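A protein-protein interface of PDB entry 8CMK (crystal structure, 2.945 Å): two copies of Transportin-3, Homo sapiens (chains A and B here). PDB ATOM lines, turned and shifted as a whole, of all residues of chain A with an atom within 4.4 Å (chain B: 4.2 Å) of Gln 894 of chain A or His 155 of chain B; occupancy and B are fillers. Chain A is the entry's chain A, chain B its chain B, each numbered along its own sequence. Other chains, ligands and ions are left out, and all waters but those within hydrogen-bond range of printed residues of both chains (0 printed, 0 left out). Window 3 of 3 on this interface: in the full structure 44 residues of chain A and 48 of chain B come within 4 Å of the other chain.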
ATOM      1  N   THR A 889       8.161 -15.189  19.248  1.00  0.00           N
ATOM      2  CA  THR A 889       9.330 -15.590  18.474  1.00  0.00           C
ATOM      3  C   THR A 889       9.307 -17.086  18.139  1.00  0.00           C
ATOM      4  O   THR A 889       9.857 -17.476  17.106  1.00  0.00           O
ATOM      5  CB  THR A 889      10.613 -15.152  19.199  1.00  0.00           C
ATOM      6  OG1 THR A 889      10.535 -15.520  20.577  1.00  0.00           O
ATOM      7  CG2 THR A 889      10.849 -13.659  19.112  1.00  0.00           C
ATOM      8  N   VAL A 890       8.680 -17.921  18.997  1.00  0.00           N
ATOM      9  CA  VAL A 890       8.451 -19.331  18.676  1.00  0.00           C
ATOM     10  C   VAL A 890       6.964 -19.692  18.725  1.00  0.00           C
ATOM     11  O   VAL A 890       6.189 -19.172  19.533  1.00  0.00           O
ATOM     12  CB  VAL A 890       9.272 -20.306  19.550  1.00  0.00           C
ATOM     13  CG1 VAL A 890      10.760 -20.185  19.266  1.00  0.00           C
ATOM     14  CG2 VAL A 890       9.002 -20.170  21.047  1.00  0.00           C
ATOM     15  N   THR A 891       6.596 -20.645  17.855  1.00  0.00           N
ATOM     16  CA  THR A 891       5.241 -21.173  17.778  1.00  0.00           C
ATOM     17  C   THR A 891       5.202 -22.614  18.296  1.00  0.00           C
ATOM     18  O   THR A 891       6.186 -23.337  18.193  1.00  0.00           O
ATOM     19  CB  THR A 891       4.681 -21.062  16.349  1.00  0.00           C
ATOM     20  OG1 THR A 891       3.311 -21.466  16.389  1.00  0.00           O
ATOM     21  CG2 THR A 891       5.406 -21.897  15.313  1.00  0.00           C
ATOM     22  N   HIS A 892       4.035 -23.024  18.819  1.00  0.00           N
ATOM     23  CA  HIS A 892       3.760 -24.363  19.330  1.00  0.00           C
ATOM     24  C   HIS A 892       4.269 -25.456  18.381  1.00  0.00           C
ATOM     25  O   HIS A 892       4.743 -26.511  18.817  1.00  0.00           O
ATOM     26  CB  HIS A 892       2.252 -24.461  19.602  1.00  0.00           C
ATOM     27  CG  HIS A 892       1.778 -25.754  20.167  1.00  0.00           C
ATOM     28  ND1 HIS A 892       1.623 -25.967  21.519  1.00  0.00           N
ATOM     29  CD2 HIS A 892       1.469 -26.909  19.565  1.00  0.00           C
ATOM     30  CE1 HIS A 892       1.218 -27.218  21.717  1.00  0.00           C
ATOM     31  NE2 HIS A 892       1.136 -27.812  20.541  1.00  0.00           N
ATOM     32  N   LYS A 893       4.212 -25.191  17.072  1.00  0.00           N
ATOM     33  CA  LYS A 893       4.646 -26.164  16.082  1.00  0.00           C
ATOM     34  C   LYS A 893       6.168 -26.368  16.124  1.00  0.00           C
ATOM     35  O   LYS A 893       6.633 -27.503  16.020  1.00  0.00           O
ATOM     36  CB  LYS A 893       4.132 -25.738  14.704  1.00  0.00           C
ATOM     37  CG  LYS A 893       4.249 -26.807  13.631  1.00  0.00           C
ATOM     38  CD  LYS A 893       5.453 -26.642  12.736  1.00  0.00           C
ATOM     39  CE  LYS A 893       5.571 -27.762  11.722  1.00  0.00           C
ATOM     40  NZ  LYS A 893       6.784 -27.625  10.883  1.00  0.00           N
ATOM     41  N   GLN A 894       6.950 -25.289  16.295  1.00  0.00           N
ATOM     42  CA  GLN A 894       8.397 -25.391  16.457  1.00  0.00           C
ATOM     43  C   GLN A 894       8.759 -26.109  17.763  1.00  0.00           C
ATOM     44  O   GLN A 894       9.716 -26.877  17.777  1.00  0.00           O
ATOM     45  CB  GLN A 894       9.065 -24.012  16.466  1.00  0.00           C
ATOM     46  CG  GLN A 894       9.110 -23.305  15.113  1.00  0.00           C
ATOM     47  CD  GLN A 894       9.332 -21.816  15.261  1.00  0.00           C
ATOM     48  OE1 GLN A 894       8.748 -21.172  16.134  1.00  0.00           O
ATOM     49  NE2 GLN A 894      10.188 -21.257  14.418  1.00  0.00           N
ATOM     50  N   LEU A 895       8.017 -25.865  18.857  1.00  0.00           N
ATOM     51  CA  LEU A 895       8.235 -26.584  20.112  1.00  0.00           C
ATOM     52  C   LEU A 895       8.049 -28.084  19.892  1.00  0.00           C
ATOM     53  O   LEU A 895       8.843 -28.901  20.356  1.00  0.00           O
ATOM     54  CB  LEU A 895       7.248 -26.120  21.187  1.00  0.00           C
ATOM     55  CG  LEU A 895       7.215 -24.626  21.506  1.00  0.00           C
ATOM     56  CD1 LEU A 895       6.172 -24.346  22.582  1.00  0.00           C
ATOM     57  CD2 LEU A 895       8.585 -24.106  21.939  1.00  0.00           C
ATOM     58  N   THR A 896       6.979 -28.427  19.176  1.00  0.00           N
ATOM     59  CA  THR A 896       6.589 -29.801  18.933  1.00  0.00           C
ATOM     60  C   THR A 896       7.549 -30.468  17.949  1.00  0.00           C
ATOM     61  O   THR A 896       7.883 -31.632  18.119  1.00  0.00           O
ATOM     62  CB  THR A 896       5.134 -29.826  18.457  1.00  0.00           C
ATOM     63  OG1 THR A 896       4.365 -29.199  19.485  1.00  0.00           O
ATOM     64  CG2 THR A 896       4.604 -31.216  18.183  1.00  0.00           C
ATOM     65  N   ASP A 897       8.017 -29.736  16.937  1.00  0.00           N
ATOM     66  CA  ASP A 897       9.015 -30.240  15.998  1.00  0.00           C
ATOM     67  C   ASP A 897      10.347 -30.540  16.695  1.00  0.00           C
ATOM     68  O   ASP A 897      11.012 -31.525  16.385  1.00  0.00           O
ATOM     69  CB  ASP A 897       9.257 -29.227  14.876  1.00  0.00           C
ATOM     70  CG  ASP A 897       8.098 -28.982  13.917  1.00  0.00           C
ATOM     71  OD1 ASP A 897       7.155 -29.808  13.854  1.00  0.00           O
ATOM     72  OD2 ASP A 897       8.144 -27.942  13.232  1.00  0.00           O
ATOM     73  N   PHE A 898      10.758 -29.667  17.619  1.00  0.00           N
ATOM     74  CA  PHE A 898      11.992 -29.849  18.369  1.00  0.00           C
ATOM     75  C   PHE A 898      11.879 -31.037  19.325  1.00  0.00           C
ATOM     76  O   PHE A 898      12.745 -31.901  19.358  1.00  0.00           O
ATOM     77  CB  PHE A 898      12.318 -28.562  19.118  1.00  0.00           C
ATOM     78  CG  PHE A 898      13.244 -28.762  20.284  1.00  0.00           C
ATOM     79  CD1 PHE A 898      14.601 -28.979  20.089  1.00  0.00           C
ATOM     80  CD2 PHE A 898      12.744 -28.778  21.572  1.00  0.00           C
ATOM     81  CE1 PHE A 898      15.452 -29.146  21.171  1.00  0.00           C
ATOM     82  CE2 PHE A 898      13.595 -28.942  22.652  1.00  0.00           C
ATOM     83  CZ  PHE A 898      14.947 -29.115  22.453  1.00  0.00           C
ATOM     84  N   LEU A 921      16.610 -19.739  17.891  1.00  0.00           N
ATOM     85  CA  LEU A 921      15.329 -19.046  17.954  1.00  0.00           C
ATOM     86  C   LEU A 921      15.224 -18.109  19.167  1.00  0.00           C
ATOM     87  O   LEU A 921      14.180 -17.483  19.340  1.00  0.00           O
ATOM     88  CB  LEU A 921      14.208 -20.099  17.973  1.00  0.00           C
ATOM     89  CG  LEU A 921      14.178 -21.076  16.793  1.00  0.00           C
ATOM     90  CD1 LEU A 921      13.236 -22.245  17.054  1.00  0.00           C
ATOM     91  CD2 LEU A 921      13.773 -20.359  15.518  1.00  0.00           C
ATOM     92  N   GLU B 153       4.448 -22.034   8.042  1.00  0.00           N
ATOM     93  CA  GLU B 153       5.794 -22.326   7.554  1.00  0.00           C
ATOM     94  C   GLU B 153       6.678 -21.071   7.395  1.00  0.00           C
ATOM     95  O   GLU B 153       7.878 -21.225   7.154  1.00  0.00           O
ATOM     96  CB  GLU B 153       5.718 -23.275   6.351  1.00  0.00           C
ATOM     97  CG  GLU B 153       5.213 -24.661   6.761  1.00  0.00           C
ATOM     98  CD  GLU B 153       5.979 -25.326   7.900  1.00  0.00           C
ATOM     99  OE1 GLU B 153       7.211 -25.166   7.940  1.00  0.00           O
ATOM    100  OE2 GLU B 153       5.359 -26.035   8.737  1.00  0.00           O
ATOM    101  N   VAL B 154       6.165 -19.857   7.674  1.00  0.00           N
ATOM    102  CA  VAL B 154       7.011 -18.764   8.164  1.00  0.00           C
ATOM    103  C   VAL B 154       7.817 -19.301   9.351  1.00  0.00           C
ATOM    104  O   VAL B 154       7.279 -20.070  10.137  1.00  0.00           O
ATOM    105  CB  VAL B 154       6.190 -17.530   8.602  1.00  0.00           C
ATOM    106  CG1 VAL B 154       7.017 -16.508   9.375  1.00  0.00           C
ATOM    107  CG2 VAL B 154       5.517 -16.833   7.436  1.00  0.00           C
ATOM    108  N   HIS B 155       9.103 -18.932   9.472  1.00  0.00           N
ATOM    109  CA  HIS B 155      10.006 -19.350  10.551  1.00  0.00           C
ATOM    110  C   HIS B 155      10.065 -20.872  10.801  1.00  0.00           C
ATOM    111  O   HIS B 155      10.453 -21.281  11.897  1.00  0.00           O
ATOM    112  CB  HIS B 155       9.824 -18.501  11.832  1.00  0.00           C
ATOM    113  CG  HIS B 155       8.489 -18.464  12.533  1.00  0.00           C
ATOM    114  ND1 HIS B 155       7.925 -17.326  13.077  1.00  0.00           N
ATOM    115  CD2 HIS B 155       7.643 -19.456  12.826  1.00  0.00           C
ATOM    116  CE1 HIS B 155       6.758 -17.630  13.631  1.00  0.00           C
ATOM    117  NE2 HIS B 155       6.569 -18.918  13.488  1.00  0.00           N
ATOM    118  N   SER B 156       9.774 -21.737   9.804  1.00  0.00           N
ATOM    119  CA  SER B 156       9.535 -23.153  10.103  1.00  0.00           C
ATOM    120  C   SER B 156      10.128 -24.119   9.052  1.00  0.00           C
ATOM    121  O   SER B 156      10.646 -23.690   8.016  1.00  0.00           O
ATOM    122  CB  SER B 156       8.043 -23.335  10.420  1.00  0.00           C
ATOM    123  OG  SER B 156       7.588 -24.681  10.416  1.00  0.00           O
ATOM    124  N   ILE B 161      15.084 -21.619   8.305  1.00  0.00           N
ATOM    125  CA  ILE B 161      14.178 -20.827   9.140  1.00  0.00           C
ATOM    126  C   ILE B 161      13.859 -19.463   8.507  1.00  0.00           C
ATOM    127  O   ILE B 161      12.714 -19.003   8.573  1.00  0.00           O
ATOM    128  CB  ILE B 161      14.751 -20.704  10.574  1.00  0.00           C
ATOM    129  CG1 ILE B 161      14.916 -22.076  11.242  1.00  0.00           C
ATOM    130  CG2 ILE B 161      13.923 -19.766  11.452  1.00  0.00           C
ATOM    131  CD1 ILE B 161      13.629 -22.869  11.381  1.00  0.00           C
ATOM    132  N   LEU B 211      -0.660 -18.393  15.270  1.00  0.00           N
ATOM    133  CA  LEU B 211       0.319 -17.316  15.130  1.00  0.00           C
ATOM    134  C   LEU B 211      -0.174 -16.006  15.775  1.00  0.00           C
ATOM    135  O   LEU B 211       0.413 -14.950  15.552  1.00  0.00           O
ATOM    136  CB  LEU B 211       0.642 -17.136  13.635  1.00  0.00           C
ATOM    137  CG  LEU B 211       1.557 -18.184  12.987  1.00  0.00           C
ATOM    138  CD1 LEU B 211       2.787 -18.460  13.841  1.00  0.00           C
ATOM    139  CD2 LEU B 211       0.824 -19.485  12.681  1.00  0.00           C
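No position is printed for both chains.
OE2 of Glu 153 of chain B is in salt-bridge range of NZ of Lys 893 of chain A.
The side-chain hydroxyl of Ser 156 of chain B lies within hydrogen-bond range of the side-chain amino group of Lys 893 of chain A (3.1 Å).
NE2 of Gln 894 of chain A is in hydrogen-bond range of O of His 155 of chain B.
Printed residues of chain B that touch a printed residue of chain A: Glu 153, His 155, Ser 156 and Leu 211.
Hydrophobic or aromatic side chains of chain B within 4 Å of the printed part of chain A: His 155 and Leu 211.
Among the printed residues, 5 pairs touch across the chains.
N of Thr 891 of chain A sits at hydrogen-bond distance from OE1 of Gln 894 of chain A (2.8 Å).
The side-chain amino group of Lys 893 of chain A lies within salt-bridge range of the side-chain carboxylate of Asp 897 of chain A, 2.7 Å away.
OE1 of Glu 153 of chain B lies within hydrogen-bond range of OG of Ser 156 of chain B (2.6 Å).
Of the printed residues of chain B, Lys 893 of chain A touches Glu 153 and Ser 156.
Gln 894 of chain A touches just one residue of chain B: His 155.
Asp 897 of chain A touches none of the printed residues of chain B.
Printed residues of chain A within 4 Å of Glu 153 of chain B: Lys 893.
Of chain A, only Thr 891 (3.7 Å) and Gln 894 (2.5 Å) come within 4 Å of His 155 of chain B.
The nearest printed residue of chain A that does not touch His 155 of chain B is Thr 889 of chain A (4.5 Å).
Among the printed residues, merely in contact across the chains: Thr 891 of chain A with His 155 of chain B (3.7 Å) and Thr 891 of chain A with Leu 211 of chain B (3.98 Å).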
